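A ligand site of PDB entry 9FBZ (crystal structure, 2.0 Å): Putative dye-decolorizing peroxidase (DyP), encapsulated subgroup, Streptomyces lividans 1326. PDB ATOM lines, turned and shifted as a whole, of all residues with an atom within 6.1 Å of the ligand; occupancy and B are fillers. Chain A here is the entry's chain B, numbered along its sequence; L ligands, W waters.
Asp 146 touches the ligand (OD2 to C17, 3.7 Å).
CD1 of Leu 148 touches C17 of the ligand (3.97 Å).
CB of Phe 150 touches C9 of the ligand, 3.9 Å away.
Val 151 touches the ligand.
OD2 of Asp 152 touches C2 of the ligand, 3.5 Å away.
Gln 184 touches the ligand.
Tyr 186 touches the ligand (OH to C24, 3.7 Å).
CE1 of His 188 touches C19 of the ligand (3.5 Å).
CD of Arg 207 touches C10 of the ligand (3.6 Å).
Val 226 touches the ligand.
Thr 229 touches the ligand (OG1 to C28, 3.3 Å).
Ser 230 touches the ligand (OG to O4, 3.7 Å).
Asn 245 touches the ligand.
Thr 258 touches the ligand (OG1 to C17, 3.7 Å).
CE1 of Phe 260 touches C21 of the ligand, 3.3 Å away.
CE of Met 273 touches C31 of the ligand (3.9 Å).
CD2 of Leu 274 touches C26 of the ligand (3.7 Å).
Met 277 touches the ligand.
Ile 289 touches the ligand.
Ser 293 touches the ligand (OG to C19, 3.9 Å).
Hydrophobic or aromatic side chains within 4 Å of the ligand: Leu 148, Phe 150, Tyr 186, His 188, His 225, Val 226, Phe 260, Met 273, Leu 274, Met 277 and Ile 289.
25 residues have an atom within 4 Å of the ligand: Asp 146, Leu 148, Phe 150, Val 151, Asp 152, Gly 153, Thr 154, Glu 155, Gln 184, Tyr 186, His 188, Arg 207, His 225, Val 226, Thr 229, Ser 230, Arg 243, Asn 245, Thr 258, Phe 260, Met 273, Leu 274, Met 277, Ile 289 and Ser 293.
NE2 of His 225 is bound to FE1 of the ligand, 2.2 Å away.
The guanidinium group of Arg 243 lies within salt-bridge range of an oxygen (O1) of the ligand (2.8 Å).
An oxygen (O2) of the ligand lies within hydrogen-bond range of the backbone NH (N) of Glu 155 (3.1 Å).
The backbone NH (N) of Thr 154 is in hydrogen-bond range of an oxygen (O1) of the ligand, 3.4 Å away.
O1 of the ligand lies within hydrogen-bond range of N of Gly 153.
Water W2 lies within hydrogen-bond range of an oxygen (O2) of the ligand (2.7 Å) and the guanidinium group of Arg 207 (2.9 Å).
Water W1 lies within hydrogen-bond range of an oxygen (O4) of the ligand (2.8 Å) and the backbone carbonyl oxygen of Thr 229 (3.0 Å).
The backbone NH (N) of Phe 150 lies within hydrogen-bond range of the side-chain carboxylate (OD1) of Asp 146 (3.4 Å).
The backbone carbonyl oxygen of Thr 258 is in hydrogen-bond range of the backbone NH of Tyr 186 (2.9 Å).
The side-chain amide oxygen (OE1) of Gln 184 lies within hydrogen-bond range of the side-chain hydroxyl (OH) of Tyr 186 (2.7 Å).
The side-chain hydroxyl of Ser 230 sits at hydrogen-bond distance from the backbone carbonyl oxygen of Val 226, at 2.7 Å.
The side-chain carboxylate (OD1) of Asp 146 sits at hydrogen-bond distance from the backbone NH (N) of Leu 148.
The backbone carbonyl oxygen of Ile 289 is in hydrogen-bond range of the side-chain hydroxyl of Ser 293 (2.8 Å).
OG1 of Thr 258 lies within hydrogen-bond range of NE2 of His 188 (2.7 Å).
O of Gln 184 is in hydrogen-bond range of N of Phe 260 (2.9 Å).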
ATOM      1  N   ASP A 146      25.723  -4.648   4.527  1.00  0.00           N
ATOM      2  CA  ASP A 146      25.924  -3.810   3.382  1.00  0.00           C
ATOM      3  C   ASP A 146      26.900  -2.685   3.745  1.00  0.00           C
ATOM      4  O   ASP A 146      27.439  -2.659   4.846  1.00  0.00           O
ATOM      5  CB  ASP A 146      24.578  -3.345   2.810  1.00  0.00           C
ATOM      6  CG  ASP A 146      23.704  -2.533   3.745  1.00  0.00           C
ATOM      7  OD1 ASP A 146      24.275  -1.867   4.646  1.00  0.00           O
ATOM      8  OD2 ASP A 146      22.427  -2.559   3.540  1.00  0.00           O
ATOM      9  N   LEU A 148      26.312   0.352   4.505  1.00  0.00           N
ATOM     10  CA  LEU A 148      25.818   1.140   5.666  1.00  0.00           C
ATOM     11  C   LEU A 148      26.028   0.434   7.003  1.00  0.00           C
ATOM     12  O   LEU A 148      25.841   1.033   8.057  1.00  0.00           O
ATOM     13  CB  LEU A 148      24.337   1.464   5.459  1.00  0.00           C
ATOM     14  CG  LEU A 148      24.003   2.274   4.198  1.00  0.00           C
ATOM     15  CD1 LEU A 148      22.558   2.681   4.122  1.00  0.00           C
ATOM     16  CD2 LEU A 148      24.868   3.530   4.061  1.00  0.00           C
ATOM     17  N   PHE A 150      24.467  -2.386   8.025  1.00  0.00           N
ATOM     18  CA  PHE A 150      23.278  -3.120   8.439  1.00  0.00           C
ATOM     19  C   PHE A 150      23.187  -4.450   7.680  1.00  0.00           C
ATOM     20  O   PHE A 150      23.556  -4.542   6.494  1.00  0.00           O
ATOM     21  CB  PHE A 150      22.017  -2.271   8.156  1.00  0.00           C
ATOM     22  CG  PHE A 150      21.746  -1.208   9.183  1.00  0.00           C
ATOM     23  CD1 PHE A 150      22.605  -0.117   9.313  1.00  0.00           C
ATOM     24  CD2 PHE A 150      20.758  -1.389  10.145  1.00  0.00           C
ATOM     25  CE1 PHE A 150      22.423   0.793  10.344  1.00  0.00           C
ATOM     26  CE2 PHE A 150      20.563  -0.470  11.161  1.00  0.00           C
ATOM     27  CZ  PHE A 150      21.397   0.645  11.248  1.00  0.00           C
ATOM     28  N   VAL A 151      22.669  -5.468   8.361  1.00  0.00           N
ATOM     29  CA  VAL A 151      22.371  -6.749   7.746  1.00  0.00           C
ATOM     30  C   VAL A 151      21.331  -6.509   6.649  1.00  0.00           C
ATOM     31  O   VAL A 151      20.348  -5.775   6.860  1.00  0.00           O
ATOM     32  CB  VAL A 151      21.870  -7.768   8.802  1.00  0.00           C
ATOM     33  CG1 VAL A 151      21.561  -9.114   8.155  1.00  0.00           C
ATOM     34  CG2 VAL A 151      22.852  -7.915   9.955  1.00  0.00           C
ATOM     35  N   ASP A 152      21.540  -7.107   5.490  1.00  0.00           N
ATOM     36  CA  ASP A 152      20.813  -6.779   4.288  1.00  0.00           C
ATOM     37  C   ASP A 152      20.327  -8.076   3.619  1.00  0.00           C
ATOM     38  O   ASP A 152      21.149  -8.850   3.137  1.00  0.00           O
ATOM     39  CB  ASP A 152      21.691  -5.939   3.352  1.00  0.00           C
ATOM     40  CG  ASP A 152      20.938  -5.210   2.237  1.00  0.00           C
ATOM     41  OD1 ASP A 152      20.007  -5.792   1.676  1.00  0.00           O
ATOM     42  OD2 ASP A 152      21.373  -4.066   1.913  1.00  0.00           O
ATOM     43  N   GLY A 153      18.981  -8.255   3.553  1.00  0.00           N
ATOM     44  CA  GLY A 153      18.331  -9.421   2.985  1.00  0.00           C
ATOM     45  C   GLY A 153      17.414 -10.197   3.962  1.00  0.00           C
ATOM     46  O   GLY A 153      16.699 -11.119   3.578  1.00  0.00           O
ATOM     47  N   THR A 154      17.395  -9.812   5.236  1.00  0.00           N
ATOM     48  CA  THR A 154      16.756 -10.599   6.302  1.00  0.00           C
ATOM     49  C   THR A 154      15.285 -10.929   5.990  1.00  0.00           C
ATOM     50  O   THR A 154      14.856 -12.014   6.246  1.00  0.00           O
ATOM     51  CB  THR A 154      16.788  -9.786   7.598  1.00  0.00           C
ATOM     52  OG1 THR A 154      18.152  -9.311   7.740  1.00  0.00           O
ATOM     53  CG2 THR A 154      16.272 -10.555   8.797  1.00  0.00           C
ATOM     54  N   GLU A 155      14.482  -9.969   5.546  1.00  0.00           N
ATOM     55  CA  GLU A 155      13.043 -10.182   5.323  1.00  0.00           C
ATOM     56  C   GLU A 155      12.731 -10.637   3.898  1.00  0.00           C
ATOM     57  O   GLU A 155      11.575 -10.690   3.562  1.00  0.00           O
ATOM     58  CB  GLU A 155      12.239  -8.925   5.685  1.00  0.00           C
ATOM     59  CG  GLU A 155      12.140  -8.696   7.211  1.00  0.00           C
ATOM     60  CD  GLU A 155      11.470  -9.839   7.958  1.00  0.00           C
ATOM     61  OE1 GLU A 155      10.348 -10.149   7.624  1.00  0.00           O
ATOM     62  OE2 GLU A 155      12.118 -10.458   8.779  1.00  0.00           O
ATOM     63  N   ASN A 156      13.748 -11.028   3.085  1.00  0.00           N
ATOM     64  CA  ASN A 156      13.421 -11.647   1.822  1.00  0.00           C
ATOM     65  C   ASN A 156      12.528 -12.871   2.076  1.00  0.00           C
ATOM     66  O   ASN A 156      12.780 -13.652   3.004  1.00  0.00           O
ATOM     67  CB  ASN A 156      14.624 -12.162   1.049  1.00  0.00           C
ATOM     68  CG  ASN A 156      15.288 -11.132   0.165  1.00  0.00           C
ATOM     69  OD1 ASN A 156      14.650 -10.234  -0.360  1.00  0.00           O
ATOM     70  ND2 ASN A 156      16.602 -11.210   0.034  1.00  0.00           N
ATOM     71  N   GLN A 184      18.998  -0.432  -9.706  1.00  0.00           N
ATOM     72  CA  GLN A 184      19.454   0.922  -9.470  1.00  0.00           C
ATOM     73  C   GLN A 184      20.809   0.906  -8.767  1.00  0.00           C
ATOM     74  O   GLN A 184      20.975   0.289  -7.719  1.00  0.00           O
ATOM     75  CB  GLN A 184      18.499   1.709  -8.558  1.00  0.00           C
ATOM     76  CG  GLN A 184      17.056   1.843  -9.004  1.00  0.00           C
ATOM     77  CD  GLN A 184      16.283   2.608  -7.977  1.00  0.00           C
ATOM     78  OE1 GLN A 184      16.017   2.088  -6.893  1.00  0.00           O
ATOM     79  NE2 GLN A 184      16.012   3.879  -8.273  1.00  0.00           N
ATOM     80  N   TYR A 186      23.338   2.808  -6.498  1.00  0.00           N
ATOM     81  CA  TYR A 186      23.317   3.877  -5.524  1.00  0.00           C
ATOM     82  C   TYR A 186      24.721   4.167  -5.025  1.00  0.00           C
ATOM     83  O   TYR A 186      25.475   3.235  -4.731  1.00  0.00           O
ATOM     84  CB  TYR A 186      22.451   3.549  -4.295  1.00  0.00           C
ATOM     85  CG  TYR A 186      20.938   3.598  -4.486  1.00  0.00           C
ATOM     86  CD1 TYR A 186      20.242   4.765  -4.263  1.00  0.00           C
ATOM     87  CD2 TYR A 186      20.208   2.469  -4.861  1.00  0.00           C
ATOM     88  CE1 TYR A 186      18.859   4.819  -4.435  1.00  0.00           C
ATOM     89  CE2 TYR A 186      18.826   2.497  -4.997  1.00  0.00           C
ATOM     90  CZ  TYR A 186      18.146   3.673  -4.789  1.00  0.00           C
ATOM     91  OH  TYR A 186      16.801   3.763  -4.953  1.00  0.00           O
ATOM     92  N   HIS A 188      26.703   6.311  -1.874  1.00  0.00           N
ATOM     93  CA  HIS A 188      26.409   6.764  -0.538  1.00  0.00           C
ATOM     94  C   HIS A 188      27.339   7.914  -0.183  1.00  0.00           C
ATOM     95  O   HIS A 188      28.512   7.936  -0.583  1.00  0.00           O
ATOM     96  CB  HIS A 188      26.563   5.611   0.459  1.00  0.00           C
ATOM     97  CG  HIS A 188      25.557   4.532   0.290  1.00  0.00           C
ATOM     98  ND1 HIS A 188      24.207   4.736   0.419  1.00  0.00           N
ATOM     99  CD2 HIS A 188      25.717   3.229  -0.015  1.00  0.00           C
ATOM    100  CE1 HIS A 188      23.586   3.566   0.140  1.00  0.00           C
ATOM    101  NE2 HIS A 188      24.494   2.643  -0.107  1.00  0.00           N
ATOM    102  N   ILE A 205      16.766   3.194   9.162  1.00  0.00           N
ATOM    103  CA  ILE A 205      16.538   1.869   8.568  1.00  0.00           C
ATOM    104  C   ILE A 205      15.229   1.277   9.092  1.00  0.00           C
ATOM    105  O   ILE A 205      14.431   0.817   8.309  1.00  0.00           O
ATOM    106  CB  ILE A 205      17.732   0.934   8.845  1.00  0.00           C
ATOM    107  CG1 ILE A 205      19.050   1.475   8.262  1.00  0.00           C
ATOM    108  CG2 ILE A 205      17.438  -0.488   8.375  1.00  0.00           C
ATOM    109  CD1 ILE A 205      18.996   1.627   6.727  1.00  0.00           C
ATOM    110  N   ARG A 207      15.461  -0.941  11.973  1.00  0.00           N
ATOM    111  CA  ARG A 207      15.912  -2.160  12.637  1.00  0.00           C
ATOM    112  C   ARG A 207      17.116  -1.802  13.501  1.00  0.00           C
ATOM    113  O   ARG A 207      17.783  -0.846  13.210  1.00  0.00           O
ATOM    114  CB  ARG A 207      16.336  -3.245  11.630  1.00  0.00           C
ATOM    115  CG  ARG A 207      15.275  -3.601  10.604  1.00  0.00           C
ATOM    116  CD  ARG A 207      15.726  -4.719   9.646  1.00  0.00           C
ATOM    117  NE  ARG A 207      15.719  -6.059  10.294  1.00  0.00           N
ATOM    118  CZ  ARG A 207      14.612  -6.798  10.466  1.00  0.00           C
ATOM    119  NH1 ARG A 207      14.598  -7.781  11.328  1.00  0.00           N
ATOM    120  NH2 ARG A 207      13.523  -6.523   9.798  1.00  0.00           N
ATOM    121  N   ASP A 212      19.837  -6.791  14.475  1.00  0.00           N
ATOM    122  CA  ASP A 212      18.950  -6.902  13.321  1.00  0.00           C
ATOM    123  C   ASP A 212      17.534  -7.246  13.783  1.00  0.00           C
ATOM    124  O   ASP A 212      16.767  -7.757  13.001  1.00  0.00           O
ATOM    125  CB  ASP A 212      19.438  -7.950  12.347  1.00  0.00           C
ATOM    126  CG  ASP A 212      18.828  -7.923  10.958  1.00  0.00           C
ATOM    127  OD1 ASP A 212      18.330  -6.868  10.552  1.00  0.00           O
ATOM    128  OD2 ASP A 212      18.884  -8.961  10.283  1.00  0.00           O
ATOM    129  N   GLU A 214      13.808  -5.946  14.356  1.00  0.00           N
ATOM    130  CA  GLU A 214      12.946  -4.883  13.909  1.00  0.00           C
ATOM    131  C   GLU A 214      12.540  -3.984  15.101  1.00  0.00           C
ATOM    132  O   GLU A 214      12.267  -4.497  16.162  1.00  0.00           O
ATOM    133  CB  GLU A 214      11.758  -5.519  13.174  1.00  0.00           C
ATOM    134  CG  GLU A 214      10.822  -4.526  12.544  1.00  0.00           C
ATOM    135  CD  GLU A 214       9.788  -5.136  11.622  1.00  0.00           C
ATOM    136  OE1 GLU A 214       9.851  -6.328  11.387  1.00  0.00           O
ATOM    137  OE2 GLU A 214       8.999  -4.376  11.087  1.00  0.00           O
ATOM    138  N   HIS A 225      13.116   3.295   6.319  1.00  0.00           N
ATOM    139  CA  HIS A 225      13.165   2.468   5.100  1.00  0.00           C
ATOM    140  C   HIS A 225      12.222   1.286   5.187  1.00  0.00           C
ATOM    141  O   HIS A 225      11.500   0.990   4.240  1.00  0.00           O
ATOM    142  CB  HIS A 225      14.610   1.997   4.865  1.00  0.00           C
ATOM    143  CG  HIS A 225      14.803   1.257   3.625  1.00  0.00           C
ATOM    144  ND1 HIS A 225      14.460   1.779   2.405  1.00  0.00           N
ATOM    145  CD2 HIS A 225      15.312   0.026   3.390  1.00  0.00           C
ATOM    146  CE1 HIS A 225      14.716   0.858   1.459  1.00  0.00           C
ATOM    147  NE2 HIS A 225      15.264  -0.223   2.056  1.00  0.00           N
ATOM    148  N   VAL A 226      12.200   0.631   6.353  1.00  0.00           N
ATOM    149  CA  VAL A 226      11.352  -0.540   6.507  1.00  0.00           C
ATOM    150  C   VAL A 226       9.858  -0.169   6.466  1.00  0.00           C
ATOM    151  O   VAL A 226       9.062  -0.944   5.935  1.00  0.00           O
ATOM    152  CB  VAL A 226      11.737  -1.294   7.796  1.00  0.00           C
ATOM    153  CG1 VAL A 226      10.634  -2.210   8.304  1.00  0.00           C
ATOM    154  CG2 VAL A 226      13.061  -2.053   7.596  1.00  0.00           C
ATOM    155  N   THR A 229       8.796   0.650   2.763  1.00  0.00           N
ATOM    156  CA  THR A 229       8.877  -0.442   1.794  1.00  0.00           C
ATOM    157  C   THR A 229       8.010  -1.621   2.224  1.00  0.00           C
ATOM    158  O   THR A 229       8.064  -2.669   1.591  1.00  0.00           O
ATOM    159  CB  THR A 229      10.339  -0.839   1.523  1.00  0.00           C
ATOM    160  OG1 THR A 229      11.002  -1.299   2.708  1.00  0.00           O
ATOM    161  CG2 THR A 229      11.105   0.313   0.914  1.00  0.00           C
ATOM    162  N   SER A 230       7.260  -1.478   3.314  1.00  0.00           N
ATOM    163  CA  SER A 230       6.222  -2.416   3.749  1.00  0.00           C
ATOM    164  C   SER A 230       4.892  -1.989   3.134  1.00  0.00           C
ATOM    165  O   SER A 230       4.359  -0.949   3.462  1.00  0.00           O
ATOM    166  CB  SER A 230       6.110  -2.478   5.258  1.00  0.00           C
ATOM    167  OG  SER A 230       7.328  -3.001   5.788  1.00  0.00           O
ATOM    168  N   ILE A 241       8.971  -8.632  -2.474  1.00  0.00           N
ATOM    169  CA  ILE A 241       9.936  -8.760  -3.527  1.00  0.00           C
ATOM    170  C   ILE A 241      11.158  -9.489  -2.998  1.00  0.00           C
ATOM    171  O   ILE A 241      11.321  -9.616  -1.788  1.00  0.00           O
ATOM    172  CB  ILE A 241      10.341  -7.406  -4.125  1.00  0.00           C
ATOM    173  CG1 ILE A 241      11.194  -6.579  -3.170  1.00  0.00           C
ATOM    174  CG2 ILE A 241       9.118  -6.659  -4.631  1.00  0.00           C
ATOM    175  CD1 ILE A 241      11.807  -5.336  -3.850  1.00  0.00           C
ATOM    176  N   ARG A 243      15.255  -9.443  -3.090  1.00  0.00           N
ATOM    177  CA  ARG A 243      16.379  -8.529  -3.301  1.00  0.00           C
ATOM    178  C   ARG A 243      17.686  -9.290  -3.143  1.00  0.00           C
ATOM    179  O   ARG A 243      17.777 -10.225  -2.352  1.00  0.00           O
ATOM    180  CB  ARG A 243      16.373  -7.406  -2.261  1.00  0.00           C
ATOM    181  CG  ARG A 243      15.169  -6.484  -2.364  1.00  0.00           C
ATOM    182  CD  ARG A 243      14.977  -5.641  -1.128  1.00  0.00           C
ATOM    183  NE  ARG A 243      14.506  -6.427   0.021  1.00  0.00           N
ATOM    184  CZ  ARG A 243      15.194  -6.611   1.155  1.00  0.00           C
ATOM    185  NH1 ARG A 243      16.360  -6.006   1.382  1.00  0.00           N
ATOM    186  NH2 ARG A 243      14.781  -7.492   2.040  1.00  0.00           N
ATOM    187  N   ASN A 245      20.908  -7.226  -2.913  1.00  0.00           N
ATOM    188  CA  ASN A 245      21.722  -6.025  -2.913  1.00  0.00           C
ATOM    189  C   ASN A 245      23.194  -6.350  -2.645  1.00  0.00           C
ATOM    190  O   ASN A 245      23.508  -7.150  -1.765  1.00  0.00           O
ATOM    191  CB  ASN A 245      21.248  -5.039  -1.851  1.00  0.00           C
ATOM    192  CG  ASN A 245      19.829  -4.559  -2.024  1.00  0.00           C
ATOM    193  OD1 ASN A 245      19.199  -4.754  -3.070  1.00  0.00           O
ATOM    194  ND2 ASN A 245      19.328  -3.983  -0.955  1.00  0.00           N
ATOM    195  N   THR A 258      25.836   0.783  -3.016  1.00  0.00           N
ATOM    196  CA  THR A 258      24.956  -0.355  -2.997  1.00  0.00           C
ATOM    197  C   THR A 258      24.345  -0.533  -4.379  1.00  0.00           C
ATOM    198  O   THR A 258      23.717   0.384  -4.900  1.00  0.00           O
ATOM    199  CB  THR A 258      23.818  -0.185  -1.962  1.00  0.00           C
ATOM    200  OG1 THR A 258      24.359  -0.017  -0.642  1.00  0.00           O
ATOM    201  CG2 THR A 258      22.861  -1.365  -1.973  1.00  0.00           C
ATOM    202  N   PHE A 260      21.382  -2.110  -6.104  1.00  0.00           N
ATOM    203  CA  PHE A 260      20.065  -2.652  -5.781  1.00  0.00           C
ATOM    204  C   PHE A 260      19.559  -3.467  -6.952  1.00  0.00           C
ATOM    205  O   PHE A 260      19.597  -3.012  -8.097  1.00  0.00           O
ATOM    206  CB  PHE A 260      19.057  -1.543  -5.447  1.00  0.00           C
ATOM    207  CG  PHE A 260      17.617  -1.992  -5.432  1.00  0.00           C
ATOM    208  CD1 PHE A 260      17.068  -2.553  -4.286  1.00  0.00           C
ATOM    209  CD2 PHE A 260      16.825  -1.913  -6.558  1.00  0.00           C
ATOM    210  CE1 PHE A 260      15.773  -3.026  -4.283  1.00  0.00           C
ATOM    211  CE2 PHE A 260      15.540  -2.416  -6.551  1.00  0.00           C
ATOM    212  CZ  PHE A 260      15.018  -2.978  -5.422  1.00  0.00           C
ATOM    213  N   THR A 270       7.224  -3.416  -7.148  1.00  0.00           N
ATOM    214  CA  THR A 270       8.463  -2.675  -6.995  1.00  0.00           C
ATOM    215  C   THR A 270       8.232  -1.165  -7.219  1.00  0.00           C
ATOM    216  O   THR A 270       8.824  -0.332  -6.516  1.00  0.00           O
ATOM    217  CB  THR A 270       9.529  -3.222  -7.949  1.00  0.00           C
ATOM    218  OG1 THR A 270       9.565  -4.628  -7.864  1.00  0.00           O
ATOM    219  CG2 THR A 270      10.899  -2.682  -7.628  1.00  0.00           C
ATOM    220  N   MET A 273       6.660   0.584  -4.233  1.00  0.00           N
ATOM    221  CA  MET A 273       7.660   0.817  -3.196  1.00  0.00           C
ATOM    222  C   MET A 273       8.511   2.050  -3.560  1.00  0.00           C
ATOM    223  O   MET A 273       8.770   2.894  -2.692  1.00  0.00           O
ATOM    224  CB  MET A 273       8.563  -0.381  -3.003  1.00  0.00           C
ATOM    225  CG  MET A 273       7.880  -1.583  -2.386  1.00  0.00           C
ATOM    226  SD  MET A 273       8.917  -3.060  -2.413  1.00  0.00           S
ATOM    227  CE  MET A 273       7.824  -4.189  -1.552  1.00  0.00           C
ATOM    228  N   LEU A 274       8.981   2.130  -4.821  1.00  0.00           N
ATOM    229  CA  LEU A 274       9.767   3.263  -5.268  1.00  0.00           C
ATOM    230  C   LEU A 274       8.980   4.577  -5.131  1.00  0.00           C
ATOM    231  O   LEU A 274       9.565   5.603  -4.757  1.00  0.00           O
ATOM    232  CB  LEU A 274      10.214   3.042  -6.704  1.00  0.00           C
ATOM    233  CG  LEU A 274      11.369   2.041  -6.883  1.00  0.00           C
ATOM    234  CD1 LEU A 274      11.578   1.722  -8.365  1.00  0.00           C
ATOM    235  CD2 LEU A 274      12.667   2.563  -6.304  1.00  0.00           C
ATOM    236  N   MET A 277       9.072   5.622  -1.557  1.00  0.00           N
ATOM    237  CA  MET A 277      10.397   6.079  -1.141  1.00  0.00           C
ATOM    238  C   MET A 277      10.695   7.506  -1.623  1.00  0.00           C
ATOM    239  O   MET A 277      11.228   8.301  -0.865  1.00  0.00           O
ATOM    240  CB  MET A 277      11.483   5.137  -1.691  1.00  0.00           C
ATOM    241  CG  MET A 277      11.560   3.768  -0.972  1.00  0.00           C
ATOM    242  SD  MET A 277      12.810   2.687  -1.802  1.00  0.00           S
ATOM    243  CE  MET A 277      14.307   3.604  -1.484  1.00  0.00           C
ATOM    244  N   PHE A 278      10.462   7.782  -2.929  1.00  0.00           N
ATOM    245  CA  PHE A 278      10.879   9.021  -3.548  1.00  0.00           C
ATOM    246  C   PHE A 278       9.827  10.166  -3.431  1.00  0.00           C
ATOM    247  O   PHE A 278      10.222  11.334  -3.329  1.00  0.00           O
ATOM    248  CB  PHE A 278      11.282   8.767  -4.985  1.00  0.00           C
ATOM    249  CG  PHE A 278      12.604   8.104  -5.176  1.00  0.00           C
ATOM    250  CD1 PHE A 278      12.744   6.725  -5.061  1.00  0.00           C
ATOM    251  CD2 PHE A 278      13.729   8.851  -5.458  1.00  0.00           C
ATOM    252  CE1 PHE A 278      14.001   6.118  -5.133  1.00  0.00           C
ATOM    253  CE2 PHE A 278      14.959   8.233  -5.566  1.00  0.00           C
ATOM    254  CZ  PHE A 278      15.086   6.867  -5.425  1.00  0.00           C
ATOM    255  N   ILE A 289      16.597   6.899   3.950  1.00  0.00           N
ATOM    256  CA  ILE A 289      17.789   6.287   3.378  1.00  0.00           C
ATOM    257  C   ILE A 289      18.260   7.128   2.199  1.00  0.00           C
ATOM    258  O   ILE A 289      19.455   7.124   1.896  1.00  0.00           O
ATOM    259  CB  ILE A 289      17.580   4.787   3.023  1.00  0.00           C
ATOM    260  CG1 ILE A 289      18.879   3.996   3.142  1.00  0.00           C
ATOM    261  CG2 ILE A 289      16.949   4.608   1.651  1.00  0.00           C
ATOM    262  CD1 ILE A 289      18.702   2.490   2.886  1.00  0.00           C
ATOM    263  N   SER A 293      21.980   8.385   0.116  1.00  0.00           N
ATOM    264  CA  SER A 293      22.030   7.485  -1.024  1.00  0.00           C
ATOM    265  C   SER A 293      21.454   8.165  -2.281  1.00  0.00           C
ATOM    266  O   SER A 293      20.284   8.561  -2.286  1.00  0.00           O
ATOM    267  CB  SER A 293      21.253   6.190  -0.739  1.00  0.00           C
ATOM    268  OG  SER A 293      21.524   5.692   0.560  1.00  0.00           O
HETATM  269  C1  LIG L   1      14.853  -3.823   3.655  1.00  0.00           C
HETATM  270  C2  LIG L   1      18.972  -1.582   2.606  1.00  0.00           C
HETATM  271  C3  LIG L   1      17.217   0.086  -1.491  1.00  0.00           C
HETATM  272  C4  LIG L   1      13.185  -2.481  -0.663  1.00  0.00           C
HETATM  273  C5  LIG L   1      16.139  -3.313   3.729  1.00  0.00           C
HETATM  274  C6  LIG L   1      16.923  -3.492   4.867  1.00  0.00           C
HETATM  275  C7  LIG L   1      18.057  -2.874   4.563  1.00  0.00           C
HETATM  276  C8  LIG L   1      17.990  -2.312   3.247  1.00  0.00           C
HETATM  277  C9  LIG L   1      19.243  -2.832   5.453  1.00  0.00           C
HETATM  278  C10 LIG L   1      16.586  -4.203   6.167  1.00  0.00           C
HETATM  279  C11 LIG L   1      16.951  -5.727   6.268  1.00  0.00           C
HETATM  280  C12 LIG L   1      16.263  -6.509   5.200  1.00  0.00           C
HETATM  281  O1  LIG L   1      16.790  -6.692   4.101  1.00  0.00           O
HETATM  282  O2  LIG L   1      15.083  -6.926   5.413  1.00  0.00           O
HETATM  283  C13 LIG L   1      18.871  -0.935   1.413  1.00  0.00           C
HETATM  284  C14 LIG L   1      19.888  -0.087   0.808  1.00  0.00           C
HETATM  285  C15 LIG L   1      19.399   0.339  -0.348  1.00  0.00           C
HETATM  286  C16 LIG L   1      18.053  -0.205  -0.396  1.00  0.00           C
HETATM  287  C17 LIG L   1      21.253   0.145   1.359  1.00  0.00           C
HETATM  288  C18 LIG L   1      19.803   1.268  -1.380  1.00  0.00           C
HETATM  289  C19 LIG L   1      20.551   2.272  -1.047  1.00  0.00           C
HETATM  290  C20 LIG L   1      15.930  -0.461  -1.653  1.00  0.00           C
HETATM  291  C21 LIG L   1      15.008  -0.199  -2.663  1.00  0.00           C
HETATM  292  C22 LIG L   1      13.832  -0.908  -2.424  1.00  0.00           C
HETATM  293  C23 LIG L   1      14.070  -1.640  -1.234  1.00  0.00           C
HETATM  294  C24 LIG L   1      15.283   0.642  -3.812  1.00  0.00           C
HETATM  295  C25 LIG L   1      12.554  -1.071  -3.208  1.00  0.00           C
HETATM  296  C26 LIG L   1      12.259  -0.593  -4.372  1.00  0.00           C
HETATM  297  C27 LIG L   1      13.401  -3.035   0.590  1.00  0.00           C
HETATM  298  C28 LIG L   1      12.410  -3.927   1.192  1.00  0.00           C
HETATM  299  C29 LIG L   1      12.833  -4.285   2.336  1.00  0.00           C
HETATM  300  C30 LIG L   1      14.121  -3.645   2.482  1.00  0.00           C
HETATM  301  C31 LIG L   1      11.063  -4.369   0.626  1.00  0.00           C
HETATM  302  C32 LIG L   1      12.098  -5.210   3.303  1.00  0.00           C
HETATM  303  C33 LIG L   1      11.107  -4.461   4.276  1.00  0.00           C
HETATM  304  C34 LIG L   1      10.322  -5.368   5.206  1.00  0.00           C
HETATM  305  O3  LIG L   1      10.736  -5.569   6.376  1.00  0.00           O
HETATM  306  O4  LIG L   1       9.335  -5.925   4.697  1.00  0.00           O
HETATM  307  N1  LIG L   1      16.792  -2.567   2.744  1.00  0.00           N
HETATM  308  N2  LIG L   1      17.764  -0.831   0.755  1.00  0.00           N
HETATM  309  N3  LIG L   1      15.272  -1.240  -0.730  1.00  0.00           N
HETATM  310  N4  LIG L   1      14.403  -2.880   1.405  1.00  0.00           N
HETATM  311 FE1  LIG L   1      16.029  -1.965   1.051  1.00  0.00          FE
HETATM  312  O   HOH W   1       8.344  -5.626   2.146  1.00  0.00           O
HETATM  313  O   HOH W   2      13.442  -5.495   7.053  1.00  0.00           O
